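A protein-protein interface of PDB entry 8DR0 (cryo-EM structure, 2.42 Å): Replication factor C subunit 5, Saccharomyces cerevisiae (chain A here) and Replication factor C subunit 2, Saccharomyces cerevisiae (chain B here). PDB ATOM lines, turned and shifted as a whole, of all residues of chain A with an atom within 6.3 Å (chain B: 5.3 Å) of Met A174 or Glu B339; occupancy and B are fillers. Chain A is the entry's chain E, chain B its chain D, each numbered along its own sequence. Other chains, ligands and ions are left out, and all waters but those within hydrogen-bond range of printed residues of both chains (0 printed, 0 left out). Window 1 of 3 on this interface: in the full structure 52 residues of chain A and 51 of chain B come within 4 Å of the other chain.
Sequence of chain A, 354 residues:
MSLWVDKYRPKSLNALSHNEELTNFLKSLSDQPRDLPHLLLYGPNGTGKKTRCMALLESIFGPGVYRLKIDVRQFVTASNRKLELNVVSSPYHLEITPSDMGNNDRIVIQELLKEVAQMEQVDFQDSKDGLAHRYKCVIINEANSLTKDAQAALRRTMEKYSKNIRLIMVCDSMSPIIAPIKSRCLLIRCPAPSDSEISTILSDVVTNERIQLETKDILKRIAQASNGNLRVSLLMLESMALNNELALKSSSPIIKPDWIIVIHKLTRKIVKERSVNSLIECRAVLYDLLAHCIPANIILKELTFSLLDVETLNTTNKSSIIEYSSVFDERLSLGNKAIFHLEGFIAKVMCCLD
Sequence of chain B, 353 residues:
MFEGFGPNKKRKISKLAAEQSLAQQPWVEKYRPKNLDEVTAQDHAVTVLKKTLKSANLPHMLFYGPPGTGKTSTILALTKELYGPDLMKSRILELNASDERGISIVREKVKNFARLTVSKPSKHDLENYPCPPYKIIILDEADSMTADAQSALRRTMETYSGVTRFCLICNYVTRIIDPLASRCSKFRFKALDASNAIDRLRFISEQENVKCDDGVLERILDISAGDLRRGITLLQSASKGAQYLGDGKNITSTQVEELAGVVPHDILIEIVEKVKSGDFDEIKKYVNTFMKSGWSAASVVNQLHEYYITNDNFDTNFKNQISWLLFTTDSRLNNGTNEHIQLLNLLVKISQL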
ATOM      1  N   LEU A  40      13.613  22.498 -33.884  1.00  0.00           N
ATOM      2  CA  LEU A  40      12.507  22.323 -32.949  1.00  0.00           C
ATOM      3  C   LEU A  40      12.213  23.678 -32.321  1.00  0.00           C
ATOM      4  O   LEU A  40      12.981  24.157 -31.480  1.00  0.00           O
ATOM      5  CB  LEU A  40      12.839  21.279 -31.882  1.00  0.00           C
ATOM      6  CG  LEU A  40      11.864  21.162 -30.706  1.00  0.00           C
ATOM      7  CD1 LEU A  40      10.422  21.093 -31.186  1.00  0.00           C
ATOM      8  CD2 LEU A  40      12.201  19.946 -29.860  1.00  0.00           C
ATOM      9  N   TYR A  42      10.078  25.871 -29.899  1.00  0.00           N
ATOM     10  CA  TYR A  42       9.239  25.732 -28.718  1.00  0.00           C
ATOM     11  C   TYR A  42       8.860  27.107 -28.193  1.00  0.00           C
ATOM     12  O   TYR A  42       9.694  28.019 -28.146  1.00  0.00           O
ATOM     13  CB  TYR A  42       9.942  24.916 -27.625  1.00  0.00           C
ATOM     14  CG  TYR A  42      11.212  25.534 -27.089  1.00  0.00           C
ATOM     15  CD1 TYR A  42      12.412  25.404 -27.774  1.00  0.00           C
ATOM     16  CD2 TYR A  42      11.215  26.231 -25.888  1.00  0.00           C
ATOM     17  CE1 TYR A  42      13.576  25.959 -27.284  1.00  0.00           C
ATOM     18  CE2 TYR A  42      12.374  26.790 -25.391  1.00  0.00           C
ATOM     19  CZ  TYR A  42      13.552  26.651 -26.092  1.00  0.00           C
ATOM     20  OH  TYR A  42      14.711  27.205 -25.600  1.00  0.00           O
ATOM     21  N   ASN A 144       4.697  17.699 -29.533  1.00  0.00           N
ATOM     22  CA  ASN A 144       4.638  17.330 -28.124  1.00  0.00           C
ATOM     23  C   ASN A 144       3.562  16.290 -27.843  1.00  0.00           C
ATOM     24  O   ASN A 144       3.588  15.663 -26.779  1.00  0.00           O
ATOM     25  CB  ASN A 144       4.401  18.577 -27.268  1.00  0.00           C
ATOM     26  CG  ASN A 144       3.097  19.277 -27.598  1.00  0.00           C
ATOM     27  OD1 ASN A 144       3.086  20.299 -28.283  1.00  0.00           O
ATOM     28  ND2 ASN A 144       1.991  18.736 -27.103  1.00  0.00           N
ATOM     29  N   CYS A 171       6.290  23.117 -31.006  1.00  0.00           N
ATOM     30  CA  CYS A 171       5.682  22.659 -29.766  1.00  0.00           C
ATOM     31  C   CYS A 171       5.442  23.824 -28.816  1.00  0.00           C
ATOM     32  O   CYS A 171       6.158  24.834 -28.833  1.00  0.00           O
ATOM     33  CB  CYS A 171       6.551  21.593 -29.085  1.00  0.00           C
ATOM     34  SG  CYS A 171       8.104  22.211 -28.408  1.00  0.00           S
ATOM     35  N   ASP A 172       4.409  23.667 -27.987  1.00  0.00           N
ATOM     36  CA  ASP A 172       4.159  24.616 -26.911  1.00  0.00           C
ATOM     37  C   ASP A 172       5.126  24.401 -25.753  1.00  0.00           C
ATOM     38  O   ASP A 172       5.570  25.368 -25.123  1.00  0.00           O
ATOM     39  CB  ASP A 172       2.712  24.497 -26.430  1.00  0.00           C
ATOM     40  CG  ASP A 172       2.376  23.108 -25.920  1.00  0.00           C
ATOM     41  OD1 ASP A 172       3.268  22.234 -25.926  1.00  0.00           O
ATOM     42  OD2 ASP A 172       1.216  22.890 -25.511  1.00  0.00           O
ATOM     43  N   SER A 173       5.461  23.146 -25.462  1.00  0.00           N
ATOM     44  CA  SER A 173       6.405  22.809 -24.409  1.00  0.00           C
ATOM     45  C   SER A 173       7.230  21.610 -24.849  1.00  0.00           C
ATOM     46  O   SER A 173       6.773  20.777 -25.635  1.00  0.00           O
ATOM     47  CB  SER A 173       5.694  22.498 -23.086  1.00  0.00           C
ATOM     48  OG  SER A 173       4.790  21.417 -23.235  1.00  0.00           O
ATOM     49  N   MET A 174       8.455  21.532 -24.335  1.00  0.00           N
ATOM     50  CA  MET A 174       9.365  20.439 -24.644  1.00  0.00           C
ATOM     51  C   MET A 174       9.339  19.332 -23.598  1.00  0.00           C
ATOM     52  O   MET A 174      10.047  18.334 -23.756  1.00  0.00           O
ATOM     53  CB  MET A 174      10.793  20.975 -24.786  1.00  0.00           C
ATOM     54  CG  MET A 174      11.125  21.484 -26.179  1.00  0.00           C
ATOM     55  SD  MET A 174      12.871  21.883 -26.394  1.00  0.00           S
ATOM     56  CE  MET A 174      13.146  23.001 -25.022  1.00  0.00           C
ATOM     57  N   SER A 175       8.542  19.481 -22.541  1.00  0.00           N
ATOM     58  CA  SER A 175       8.525  18.472 -21.487  1.00  0.00           C
ATOM     59  C   SER A 175       8.143  17.087 -21.997  1.00  0.00           C
ATOM     60  O   SER A 175       8.771  16.107 -21.562  1.00  0.00           O
ATOM     61  CB  SER A 175       7.590  18.920 -20.355  1.00  0.00           C
ATOM     62  OG  SER A 175       6.267  18.453 -20.546  1.00  0.00           O
ATOM     63  N   PRO A 176       7.154  16.921 -22.883  1.00  0.00           N
ATOM     64  CA  PRO A 176       6.817  15.572 -23.360  1.00  0.00           C
ATOM     65  C   PRO A 176       7.776  15.016 -24.403  1.00  0.00           C
ATOM     66  O   PRO A 176       7.624  13.849 -24.789  1.00  0.00           O
ATOM     67  CB  PRO A 176       5.407  15.750 -23.956  1.00  0.00           C
ATOM     68  CG  PRO A 176       4.970  17.145 -23.575  1.00  0.00           C
ATOM     69  CD  PRO A 176       6.228  17.923 -23.430  1.00  0.00           C
ATOM     70  N   ILE A 177       8.743  15.798 -24.873  1.00  0.00           N
ATOM     71  CA  ILE A 177       9.685  15.329 -25.884  1.00  0.00           C
ATOM     72  C   ILE A 177      10.781  14.518 -25.205  1.00  0.00           C
ATOM     73  O   ILE A 177      11.375  14.960 -24.214  1.00  0.00           O
ATOM     74  CB  ILE A 177      10.278  16.509 -26.671  1.00  0.00           C
ATOM     75  CG1 ILE A 177       9.167  17.396 -27.242  1.00  0.00           C
ATOM     76  CG2 ILE A 177      11.183  16.003 -27.786  1.00  0.00           C
ATOM     77  CD1 ILE A 177       8.252  16.697 -28.225  1.00  0.00           C
ATOM     78  N   ILE A 178      11.054  13.326 -25.739  1.00  0.00           N
ATOM     79  CA  ILE A 178      12.088  12.476 -25.155  1.00  0.00           C
ATOM     80  C   ILE A 178      13.467  13.085 -25.398  1.00  0.00           C
ATOM     81  O   ILE A 178      13.697  13.832 -26.357  1.00  0.00           O
ATOM     82  CB  ILE A 178      12.002  11.046 -25.711  1.00  0.00           C
ATOM     83  CG1 ILE A 178      12.270  11.031 -27.221  1.00  0.00           C
ATOM     84  CG2 ILE A 178      10.639  10.446 -25.408  1.00  0.00           C
ATOM     85  CD1 ILE A 178      12.252   9.646 -27.831  1.00  0.00           C
ATOM     86  N   LYS A 182      15.273  15.648 -28.525  1.00  0.00           N
ATOM     87  CA  LYS A 182      15.813  16.976 -28.258  1.00  0.00           C
ATOM     88  C   LYS A 182      17.298  17.035 -28.588  1.00  0.00           C
ATOM     89  O   LYS A 182      17.795  18.057 -29.075  1.00  0.00           O
ATOM     90  CB  LYS A 182      15.570  17.360 -26.797  1.00  0.00           C
ATOM     91  CG  LYS A 182      14.146  17.809 -26.508  1.00  0.00           C
ATOM     92  CD  LYS A 182      13.763  17.585 -25.052  1.00  0.00           C
ATOM     93  CE  LYS A 182      14.656  18.367 -24.101  1.00  0.00           C
ATOM     94  NZ  LYS A 182      14.653  19.828 -24.391  1.00  0.00           N
ATOM     95  N   LEU A 187      17.284  23.542 -30.942  1.00  0.00           N
ATOM     96  CA  LEU A 187      16.170  24.093 -30.181  1.00  0.00           C
ATOM     97  C   LEU A 187      16.120  25.606 -30.349  1.00  0.00           C
ATOM     98  O   LEU A 187      17.139  26.287 -30.199  1.00  0.00           O
ATOM     99  CB  LEU A 187      16.300  23.730 -28.702  1.00  0.00           C
ATOM    100  CG  LEU A 187      16.604  22.261 -28.401  1.00  0.00           C
ATOM    101  CD1 LEU A 187      16.617  22.015 -26.901  1.00  0.00           C
ATOM    102  CD2 LEU A 187      15.600  21.348 -29.086  1.00  0.00           C
ATOM    103  N   ASP A 329      -2.182  17.012 -12.339  1.00  0.00           N
ATOM    104  CA  ASP A 329      -1.699  17.197 -13.701  1.00  0.00           C
ATOM    105  C   ASP A 329      -0.757  16.065 -14.091  1.00  0.00           C
ATOM    106  O   ASP A 329      -0.822  15.554 -15.217  1.00  0.00           O
ATOM    107  CB  ASP A 329      -1.017  18.560 -13.825  1.00  0.00           C
ATOM    108  CG  ASP A 329      -0.070  18.639 -15.000  1.00  0.00           C
ATOM    109  OD1 ASP A 329      -0.538  18.565 -16.154  1.00  0.00           O
ATOM    110  OD2 ASP A 329       1.144  18.794 -14.768  1.00  0.00           O
ATOM    111  N   MET B 291       6.793  32.961 -17.643  1.00  0.00           N
ATOM    112  CA  MET B 291       6.472  31.893 -18.585  1.00  0.00           C
ATOM    113  C   MET B 291       6.136  32.407 -19.978  1.00  0.00           C
ATOM    114  O   MET B 291       6.086  31.605 -20.915  1.00  0.00           O
ATOM    115  CB  MET B 291       5.312  31.045 -18.058  1.00  0.00           C
ATOM    116  CG  MET B 291       5.555  30.444 -16.676  1.00  0.00           C
ATOM    117  SD  MET B 291       6.638  28.997 -16.656  1.00  0.00           S
ATOM    118  CE  MET B 291       5.995  28.014 -18.008  1.00  0.00           C
ATOM    119  N   TRP B 295      10.982  30.171 -21.590  1.00  0.00           N
ATOM    120  CA  TRP B 295      12.080  29.423 -20.990  1.00  0.00           C
ATOM    121  C   TRP B 295      11.641  28.001 -20.660  1.00  0.00           C
ATOM    122  O   TRP B 295      10.531  27.772 -20.172  1.00  0.00           O
ATOM    123  CB  TRP B 295      12.570  30.122 -19.723  1.00  0.00           C
ATOM    124  CG  TRP B 295      13.040  31.525 -19.945  1.00  0.00           C
ATOM    125  CD1 TRP B 295      12.452  32.668 -19.491  1.00  0.00           C
ATOM    126  CD2 TRP B 295      14.204  31.934 -20.672  1.00  0.00           C
ATOM    127  NE1 TRP B 295      13.175  33.765 -19.891  1.00  0.00           N
ATOM    128  CE2 TRP B 295      14.256  33.341 -20.618  1.00  0.00           C
ATOM    129  CE3 TRP B 295      15.205  31.249 -21.364  1.00  0.00           C
ATOM    130  CZ2 TRP B 295      15.269  34.073 -21.231  1.00  0.00           C
ATOM    131  CZ3 TRP B 295      16.209  31.976 -21.971  1.00  0.00           C
ATOM    132  CH2 TRP B 295      16.234  33.374 -21.902  1.00  0.00           C
ATOM    133  N   SER B 296      12.524  27.044 -20.929  1.00  0.00           N
ATOM    134  CA  SER B 296      12.240  25.651 -20.613  1.00  0.00           C
ATOM    135  C   SER B 296      12.330  25.427 -19.109  1.00  0.00           C
ATOM    136  O   SER B 296      13.283  25.869 -18.459  1.00  0.00           O
ATOM    137  CB  SER B 296      13.216  24.734 -21.347  1.00  0.00           C
ATOM    138  OG  SER B 296      13.419  23.526 -20.635  1.00  0.00           O
ATOM    139  N   ALA B 297      11.334  24.730 -18.554  1.00  0.00           N
ATOM    140  CA  ALA B 297      11.287  24.528 -17.109  1.00  0.00           C
ATOM    141  C   ALA B 297      12.461  23.694 -16.615  1.00  0.00           C
ATOM    142  O   ALA B 297      12.958  23.924 -15.508  1.00  0.00           O
ATOM    143  CB  ALA B 297       9.968  23.867 -16.715  1.00  0.00           C
ATOM    144  N   LEU B 333       8.344  16.660 -13.973  1.00  0.00           N
ATOM    145  CA  LEU B 333       8.530  17.227 -15.304  1.00  0.00           C
ATOM    146  C   LEU B 333       8.931  16.163 -16.316  1.00  0.00           C
ATOM    147  O   LEU B 333       8.552  16.252 -17.489  1.00  0.00           O
ATOM    148  CB  LEU B 333       9.583  18.335 -15.262  1.00  0.00           C
ATOM    149  CG  LEU B 333       9.117  19.697 -14.741  1.00  0.00           C
ATOM    150  CD1 LEU B 333      10.307  20.613 -14.512  1.00  0.00           C
ATOM    151  CD2 LEU B 333       8.125  20.337 -15.701  1.00  0.00           C
ATOM    152  N   THR B 337       4.638  17.028 -17.991  1.00  0.00           N
ATOM    153  CA  THR B 337       3.608  17.767 -17.275  1.00  0.00           C
ATOM    154  C   THR B 337       3.630  19.243 -17.660  1.00  0.00           C
ATOM    155  O   THR B 337       4.562  19.737 -18.298  1.00  0.00           O
ATOM    156  CB  THR B 337       3.799  17.612 -15.763  1.00  0.00           C
ATOM    157  OG1 THR B 337       5.188  17.743 -15.437  1.00  0.00           O
ATOM    158  CG2 THR B 337       3.293  16.258 -15.297  1.00  0.00           C
ATOM    159  N   ASN B 338       2.574  19.948 -17.259  1.00  0.00           N
ATOM    160  CA  ASN B 338       2.484  21.382 -17.506  1.00  0.00           C
ATOM    161  C   ASN B 338       3.600  22.111 -16.767  1.00  0.00           C
ATOM    162  O   ASN B 338       3.710  22.016 -15.542  1.00  0.00           O
ATOM    163  CB  ASN B 338       1.117  21.901 -17.062  1.00  0.00           C
ATOM    164  CG  ASN B 338       0.921  23.371 -17.370  1.00  0.00           C
ATOM    165  OD1 ASN B 338       1.432  24.239 -16.664  1.00  0.00           O
ATOM    166  ND2 ASN B 338       0.175  23.657 -18.429  1.00  0.00           N
ATOM    167  N   GLU B 339       4.420  22.849 -17.517  1.00  0.00           N
ATOM    168  CA  GLU B 339       5.587  23.494 -16.924  1.00  0.00           C
ATOM    169  C   GLU B 339       5.187  24.614 -15.969  1.00  0.00           C
ATOM    170  O   GLU B 339       5.801  24.781 -14.909  1.00  0.00           O
ATOM    171  CB  GLU B 339       6.498  24.030 -18.028  1.00  0.00           C
ATOM    172  CG  GLU B 339       7.220  22.941 -18.806  1.00  0.00           C
ATOM    173  CD  GLU B 339       8.148  23.496 -19.870  1.00  0.00           C
ATOM    174  OE1 GLU B 339       8.479  24.698 -19.808  1.00  0.00           O
ATOM    175  OE2 GLU B 339       8.547  22.726 -20.768  1.00  0.00           O
ATOM    176  N   HIS B 340       4.166  25.392 -16.327  1.00  0.00           N
ATOM    177  CA  HIS B 340       3.761  26.526 -15.500  1.00  0.00           C
ATOM    178  C   HIS B 340       3.370  26.071 -14.097  1.00  0.00           C
ATOM    179  O   HIS B 340       3.858  26.610 -13.094  1.00  0.00           O
ATOM    180  CB  HIS B 340       2.602  27.258 -16.181  1.00  0.00           C
ATOM    181  CG  HIS B 340       2.279  28.592 -15.584  1.00  0.00           C
ATOM    182  ND1 HIS B 340       2.766  29.008 -14.364  1.00  0.00           N
ATOM    183  CD2 HIS B 340       1.508  29.606 -16.045  1.00  0.00           C
ATOM    184  CE1 HIS B 340       2.309  30.219 -14.099  1.00  0.00           C
ATOM    185  NE2 HIS B 340       1.544  30.605 -15.105  1.00  0.00           N
ATOM    186  N   ILE B 341       2.492  25.068 -14.009  1.00  0.00           N
ATOM    187  CA  ILE B 341       1.993  24.617 -12.712  1.00  0.00           C
ATOM    188  C   ILE B 341       3.133  24.061 -11.868  1.00  0.00           C
ATOM    189  O   ILE B 341       3.257  24.371 -10.676  1.00  0.00           O
ATOM    190  CB  ILE B 341       0.876  23.575 -12.908  1.00  0.00           C
ATOM    191  CG1 ILE B 341      -0.397  24.253 -13.418  1.00  0.00           C
ATOM    192  CG2 ILE B 341       0.600  22.833 -11.607  1.00  0.00           C
ATOM    193  CD1 ILE B 341      -1.370  23.302 -14.082  1.00  0.00           C
ATOM    194  N   GLN B 342       3.980  23.225 -12.472  1.00  0.00           N
ATOM    195  CA  GLN B 342       5.066  22.605 -11.719  1.00  0.00           C
ATOM    196  C   GLN B 342       6.059  23.650 -11.223  1.00  0.00           C
ATOM    197  O   GLN B 342       6.510  23.591 -10.073  1.00  0.00           O
ATOM    198  CB  GLN B 342       5.772  21.560 -12.583  1.00  0.00           C
ATOM    199  CG  GLN B 342       4.855  20.465 -13.105  1.00  0.00           C
ATOM    200  CD  GLN B 342       4.386  19.523 -12.015  1.00  0.00           C
ATOM    201  OE1 GLN B 342       5.041  19.370 -10.985  1.00  0.00           O
ATOM    202  NE2 GLN B 342       3.241  18.889 -12.236  1.00  0.00           N
ATOM    203  N   LEU B 343       6.411  24.614 -12.076  1.00  0.00           N
ATOM    204  CA  LEU B 343       7.347  25.652 -11.660  1.00  0.00           C
ATOM    205  C   LEU B 343       6.763  26.498 -10.537  1.00  0.00           C
ATOM    206  O   LEU B 343       7.462  26.826  -9.570  1.00  0.00           O
ATOM    207  CB  LEU B 343       7.726  26.526 -12.856  1.00  0.00           C
ATOM    208  CG  LEU B 343       8.718  27.657 -12.574  1.00  0.00           C
ATOM    209  CD1 LEU B 343      10.018  27.114 -11.995  1.00  0.00           C
ATOM    210  CD2 LEU B 343       8.988  28.454 -13.839  1.00  0.00           C
ATOM    211  N   LEU B 344       5.482  26.864 -10.642  1.00  0.00           N
ATOM    212  CA  LEU B 344       4.864  27.650  -9.580  1.00  0.00           C
ATOM    213  C   LEU B 344       4.842  26.876  -8.268  1.00  0.00           C
ATOM    214  O   LEU B 344       5.140  27.433  -7.204  1.00  0.00           O
ATOM    215  CB  LEU B 344       3.448  28.063  -9.983  1.00  0.00           C
ATOM    216  CG  LEU B 344       2.709  28.958  -8.984  1.00  0.00           C
ATOM    217  CD1 LEU B 344       3.497  30.229  -8.702  1.00  0.00           C
ATOM    218  CD2 LEU B 344       1.316  29.294  -9.488  1.00  0.00           C
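O of Thr B337 lies within hydrogen-bond range of OG of Ser A175, at 3.1 Å.
OD2 of Asp A329 lies within hydrogen-bond range of N of Asn B338, 3.1 Å away.
OD2 of Asp A329 sits at hydrogen-bond distance from NE2 of Gln B342, 3.3 Å away.
OE1 of Glu B339 is in hydrogen-bond range of N of Ala B297, 3.1 Å away.
The side-chain hydroxyl of Ser A173 lies within hydrogen-bond range of the side-chain carboxylate of Asp A172, 3.2 Å away.
The side-chain sulfur of Cys A171 is in hydrogen-bond range of the backbone carbonyl oxygen of Ser A173 (3.4 Å).
OD1 of Asn B338 is in hydrogen-bond range of N of Ile B341 (3.0 Å).
The side-chain amino group of Lys A182 lies within hydrogen-bond range of the side-chain sulfur of Met A174 (3.4 Å).
N of His B340 lies within hydrogen-bond range of OD1 of Asn B338, at 3.0 Å.
Ser A173 touches Glu B339.
Met A174 touches Glu B339 (N to OE2, 3.8 Å).
Ser A175 touches Glu B339 (N to OE2, 3.7 Å).
Asp A329 touches Thr B337.
Of chain B, only Glu B339 (3.8 Å) comes within 4 Å of Met A174.
Of chain A, only Ser A173, Met A174 and Ser A175 come within 4 Å of Glu B339.
Of the printed residues of chain B, Ser A175 touches Thr B337 (3.1 Å) and Glu B339 (3.7 Å).
Of the printed residues of chain A, Asn B338 touches Asp A329.
Ala B297 touches none of the printed residues of chain A.
Leu A187 touches none of the printed residues of chain B.
The nearest residue of chain B that does not touch Met A174 is Ser B296 (4.1 Å).
The nearest printed residue of chain A that does not touch Glu B339 is Asp A329 (5.9 Å).
The nearest printed residue of chain B that does not touch Ser A173 is Thr B337 (5.2 Å).
Of the 13 printed residues of chain B, 4 touch a printed residue of chain A.
Printed residues of chain B that touch a printed residue of chain A: Thr B337, Asn B338, Glu B339 and Gln B342.
Along chain B the printed residues that touch a printed residue of chain A span positions 337 to 342.
Among the printed residues, 7 pairs touch across the chains.
Among the printed residues, no Asp or Glu carboxylate lies within 4 Å of a Lys or Arg side-chain nitrogen of the other chain.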
